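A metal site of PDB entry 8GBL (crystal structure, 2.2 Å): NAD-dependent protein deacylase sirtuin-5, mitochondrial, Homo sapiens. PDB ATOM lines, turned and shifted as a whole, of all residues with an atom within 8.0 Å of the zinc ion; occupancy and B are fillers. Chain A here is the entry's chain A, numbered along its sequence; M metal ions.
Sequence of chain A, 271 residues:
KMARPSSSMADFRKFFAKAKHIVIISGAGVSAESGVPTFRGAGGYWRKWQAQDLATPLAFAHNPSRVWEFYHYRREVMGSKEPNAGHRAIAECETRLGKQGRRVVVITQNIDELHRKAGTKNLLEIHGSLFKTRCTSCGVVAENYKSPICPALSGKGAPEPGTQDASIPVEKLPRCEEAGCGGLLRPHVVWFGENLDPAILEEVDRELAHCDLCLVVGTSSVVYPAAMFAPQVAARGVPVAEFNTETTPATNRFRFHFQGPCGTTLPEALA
N of Cys 135 is in hydrogen-bond range of O of Val 140. N of Cys 176 sits at hydrogen-bond distance from O of Gly 183 (2.9 Å). N of Glu 178 lies close to SG of Cys 176. The side-chain sulfur (SG) of Cys 181 sits close to the backbone NH (N) of Gly 183 (3.4 Å). The backbone NH (N) of Val 140 lies close to the side-chain sulfur (SG) of Cys 138, at 3.7 Å. SG of Cys 135 sits close to N of Ser 137, at 3.3 Å.
Four residues have an atom within 4 Å of the zinc ion: Cys 135, Cys 138, Cys 176 and Cys 181.
The zinc ion is bound by SG of Cys 138 (2.2 Å). The side-chain sulfur (SG) of Cys 176 binds the zinc ion, at 2.3 Å. SG of Cys 135 binds the zinc ion, 2.3 Å away. SG of Cys 181 is bound to the zinc ion (2.4 Å). The zinc ion has four donor atoms within binding distance.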
ATOM      1  N   ARG A 134      14.942   4.854 -17.831  1.00  0.00           N
ATOM      2  CA  ARG A 134      13.518   4.549 -17.724  1.00  0.00           C
ATOM      3  C   ARG A 134      12.855   5.262 -18.900  1.00  0.00           C
ATOM      4  O   ARG A 134      13.094   6.442 -19.109  1.00  0.00           O
ATOM      5  CB  ARG A 134      12.930   5.030 -16.372  1.00  0.00           C
ATOM      6  CG  ARG A 134      11.468   4.592 -16.202  1.00  0.00           C
ATOM      7  CD  ARG A 134      10.983   4.638 -14.756  1.00  0.00           C
ATOM      8  NE  ARG A 134      10.528   5.947 -14.267  1.00  0.00           N
ATOM      9  CZ  ARG A 134      11.178   6.690 -13.375  1.00  0.00           C
ATOM     10  NH1 ARG A 134      12.356   6.317 -12.912  1.00  0.00           N
ATOM     11  NH2 ARG A 134      10.657   7.834 -12.954  1.00  0.00           N
ATOM     12  N   CYS A 135      12.058   4.559 -19.692  1.00  0.00           N
ATOM     13  CA  CYS A 135      11.345   5.171 -20.788  1.00  0.00           C
ATOM     14  C   CYS A 135      10.162   5.946 -20.248  1.00  0.00           C
ATOM     15  O   CYS A 135       9.435   5.418 -19.426  1.00  0.00           O
ATOM     16  CB  CYS A 135      10.915   4.120 -21.806  1.00  0.00           C
ATOM     17  SG  CYS A 135       9.988   4.810 -23.205  1.00  0.00           S
ATOM     18  N   THR A 136      10.032   7.230 -20.640  1.00  0.00           N
ATOM     19  CA  THR A 136       8.926   8.113 -20.246  1.00  0.00           C
ATOM     20  C   THR A 136       7.650   7.751 -20.976  1.00  0.00           C
ATOM     21  O   THR A 136       6.582   8.201 -20.578  1.00  0.00           O
ATOM     22  CB  THR A 136       9.260   9.628 -20.365  1.00  0.00           C
ATOM     23  OG1 THR A 136       9.558   9.955 -21.724  1.00  0.00           O
ATOM     24  CG2 THR A 136      10.416  10.049 -19.482  1.00  0.00           C
ATOM     25  N   SER A 137       7.744   6.942 -22.058  1.00  0.00           N
ATOM     26  CA  SER A 137       6.575   6.470 -22.796  1.00  0.00           C
ATOM     27  C   SER A 137       6.085   5.097 -22.285  1.00  0.00           C
ATOM     28  O   SER A 137       4.932   5.000 -21.875  1.00  0.00           O
ATOM     29  CB  SER A 137       6.855   6.402 -24.298  1.00  0.00           C
ATOM     30  OG  SER A 137       7.099   7.690 -24.821  1.00  0.00           O
ATOM     31  N   CYS A 138       6.923   4.067 -22.313  1.00  0.00           N
ATOM     32  CA  CYS A 138       6.503   2.713 -21.957  1.00  0.00           C
ATOM     33  C   CYS A 138       6.833   2.272 -20.519  1.00  0.00           C
ATOM     34  O   CYS A 138       6.297   1.255 -20.093  1.00  0.00           O
ATOM     35  CB  CYS A 138       7.019   1.701 -22.985  1.00  0.00           C
ATOM     36  SG  CYS A 138       8.799   1.338 -22.846  1.00  0.00           S
ATOM     37  N   GLY A 139       7.678   3.002 -19.773  1.00  0.00           N
ATOM     38  CA  GLY A 139       8.021   2.660 -18.391  1.00  0.00           C
ATOM     39  C   GLY A 139       9.111   1.617 -18.148  1.00  0.00           C
ATOM     40  O   GLY A 139       9.561   1.431 -17.007  1.00  0.00           O
ATOM     41  N   VAL A 140       9.578   0.962 -19.224  1.00  0.00           N
ATOM     42  CA  VAL A 140      10.641  -0.055 -19.135  1.00  0.00           C
ATOM     43  C   VAL A 140      11.916   0.538 -18.503  1.00  0.00           C
ATOM     44  O   VAL A 140      12.378   1.614 -18.912  1.00  0.00           O
ATOM     45  CB  VAL A 140      10.908  -0.794 -20.467  1.00  0.00           C
ATOM     46  CG1 VAL A 140      12.187  -1.632 -20.405  1.00  0.00           C
ATOM     47  CG2 VAL A 140       9.726  -1.706 -20.810  1.00  0.00           C
ATOM     48  N   VAL A 141      12.440  -0.181 -17.476  1.00  0.00           N
ATOM     49  CA  VAL A 141      13.684   0.158 -16.783  1.00  0.00           C
ATOM     50  C   VAL A 141      14.766  -0.748 -17.350  1.00  0.00           C
ATOM     51  O   VAL A 141      14.573  -1.955 -17.405  1.00  0.00           O
ATOM     52  CB  VAL A 141      13.567   0.033 -15.229  1.00  0.00           C
ATOM     53  CG1 VAL A 141      14.937   0.278 -14.545  1.00  0.00           C
ATOM     54  CG2 VAL A 141      12.501   0.980 -14.689  1.00  0.00           C
ATOM     55  N   ARG A 175      16.833   7.445 -26.567  1.00  0.00           N
ATOM     56  CA  ARG A 175      15.517   6.934 -26.968  1.00  0.00           C
ATOM     57  C   ARG A 175      15.433   5.438 -26.689  1.00  0.00           C
ATOM     58  O   ARG A 175      16.376   4.691 -26.936  1.00  0.00           O
ATOM     59  CB  ARG A 175      15.214   7.181 -28.483  1.00  0.00           C
ATOM     60  CG  ARG A 175      15.407   8.615 -29.039  1.00  0.00           C
ATOM     61  CD  ARG A 175      14.573   9.744 -28.394  1.00  0.00           C
ATOM     62  NE  ARG A 175      13.120   9.484 -28.417  1.00  0.00           N
ATOM     63  CZ  ARG A 175      12.193  10.427 -28.298  1.00  0.00           C
ATOM     64  NH1 ARG A 175      12.536  11.708 -28.216  1.00  0.00           N
ATOM     65  NH2 ARG A 175      10.908  10.099 -28.277  1.00  0.00           N
ATOM     66  N   CYS A 176      14.314   5.044 -26.157  1.00  0.00           N
ATOM     67  CA  CYS A 176      13.931   3.680 -25.835  1.00  0.00           C
ATOM     68  C   CYS A 176      14.116   2.759 -27.057  1.00  0.00           C
ATOM     69  O   CYS A 176      13.665   3.092 -28.144  1.00  0.00           O
ATOM     70  CB  CYS A 176      12.489   3.683 -25.337  1.00  0.00           C
ATOM     71  SG  CYS A 176      11.848   2.049 -24.901  1.00  0.00           S
ATOM     72  N   GLU A 177      14.740   1.608 -26.864  1.00  0.00           N
ATOM     73  CA  GLU A 177      14.978   0.658 -27.949  1.00  0.00           C
ATOM     74  C   GLU A 177      13.954  -0.452 -28.012  1.00  0.00           C
ATOM     75  O   GLU A 177      14.104  -1.326 -28.860  1.00  0.00           O
ATOM     76  CB  GLU A 177      16.396   0.077 -27.875  1.00  0.00           C
ATOM     77  CG  GLU A 177      17.514   1.099 -27.837  1.00  0.00           C
ATOM     78  CD  GLU A 177      18.881   0.451 -27.926  1.00  0.00           C
ATOM     79  OE1 GLU A 177      19.518   0.606 -28.991  1.00  0.00           O
ATOM     80  OE2 GLU A 177      19.281  -0.232 -26.968  1.00  0.00           O
ATOM     81  N   GLU A 178      12.921  -0.466 -27.140  1.00  0.00           N
ATOM     82  CA  GLU A 178      11.830  -1.472 -27.209  1.00  0.00           C
ATOM     83  C   GLU A 178      11.128  -1.298 -28.558  1.00  0.00           C
ATOM     84  O   GLU A 178      10.919  -0.147 -29.002  1.00  0.00           O
ATOM     85  CB  GLU A 178      10.815  -1.292 -26.074  1.00  0.00           C
ATOM     86  CG  GLU A 178      11.356  -1.569 -24.682  1.00  0.00           C
ATOM     87  CD  GLU A 178      11.583  -3.045 -24.400  1.00  0.00           C
ATOM     88  OE1 GLU A 178      10.629  -3.701 -23.931  1.00  0.00           O
ATOM     89  OE2 GLU A 178      12.699  -3.541 -24.656  1.00  0.00           O
ATOM     90  N   ALA A 179      10.843  -2.413 -29.255  1.00  0.00           N
ATOM     91  CA  ALA A 179      10.227  -2.380 -30.559  1.00  0.00           C
ATOM     92  C   ALA A 179       8.900  -1.614 -30.582  1.00  0.00           C
ATOM     93  O   ALA A 179       7.964  -1.923 -29.844  1.00  0.00           O
ATOM     94  CB  ALA A 179      10.022  -3.797 -31.069  1.00  0.00           C
ATOM     95  N   GLY A 180       8.835  -0.603 -31.459  1.00  0.00           N
ATOM     96  CA  GLY A 180       7.672   0.233 -31.665  1.00  0.00           C
ATOM     97  C   GLY A 180       7.473   1.321 -30.621  1.00  0.00           C
ATOM     98  O   GLY A 180       6.454   1.986 -30.613  1.00  0.00           O
ATOM     99  N   CYS A 181       8.437   1.525 -29.745  1.00  0.00           N
ATOM    100  CA  CYS A 181       8.241   2.570 -28.769  1.00  0.00           C
ATOM    101  C   CYS A 181       8.999   3.812 -29.208  1.00  0.00           C
ATOM    102  O   CYS A 181       8.386   4.749 -29.704  1.00  0.00           O
ATOM    103  CB  CYS A 181       8.630   2.112 -27.367  1.00  0.00           C
ATOM    104  SG  CYS A 181       8.442   3.404 -26.103  1.00  0.00           S
ATOM    105  N   GLY A 182      10.321   3.815 -29.012  1.00  0.00           N
ATOM    106  CA  GLY A 182      11.151   4.971 -29.343  1.00  0.00           C
ATOM    107  C   GLY A 182      10.872   6.191 -28.478  1.00  0.00           C
ATOM    108  O   GLY A 182      11.152   7.317 -28.897  1.00  0.00           O
ATOM    109  N   GLY A 183      10.313   5.982 -27.301  1.00  0.00           N
ATOM    110  CA  GLY A 183      10.026   7.055 -26.354  1.00  0.00           C
ATOM    111  C   GLY A 183      11.275   7.723 -25.786  1.00  0.00           C
ATOM    112  O   GLY A 183      12.372   7.175 -25.905  1.00  0.00           O
ATOM    113  N   LEU A 184      11.112   8.879 -25.165  1.00  0.00           N
ATOM    114  CA  LEU A 184      12.241   9.609 -24.576  1.00  0.00           C
ATOM    115  C   LEU A 184      12.678   8.965 -23.241  1.00  0.00           C
ATOM    116  O   LEU A 184      11.875   8.793 -22.318  1.00  0.00           O
ATOM    117  CB  LEU A 184      11.925  11.119 -24.436  1.00  0.00           C
ATOM    118  CG  LEU A 184      12.976  11.944 -23.714  1.00  0.00           C
ATOM    119  CD1 LEU A 184      14.302  12.006 -24.504  1.00  0.00           C
ATOM    120  CD2 LEU A 184      12.441  13.332 -23.361  1.00  0.00           C
ATOM    121  N   LEU A 185      13.959   8.594 -23.141  1.00  0.00           N
ATOM    122  CA  LEU A 185      14.495   8.012 -21.900  1.00  0.00           C
ATOM    123  C   LEU A 185      14.880   9.105 -20.929  1.00  0.00           C
ATOM    124  O   LEU A 185      15.317  10.196 -21.349  1.00  0.00           O
ATOM    125  CB  LEU A 185      15.745   7.139 -22.161  1.00  0.00           C
ATOM    126  CG  LEU A 185      15.572   5.861 -23.006  1.00  0.00           C
ATOM    127  CD1 LEU A 185      16.907   5.098 -23.144  1.00  0.00           C
ATOM    128  CD2 LEU A 185      14.515   4.932 -22.391  1.00  0.00           C
HETATM  129 ZN    ZN M   1       9.766   2.746 -24.258  1.00  0.00          ZN
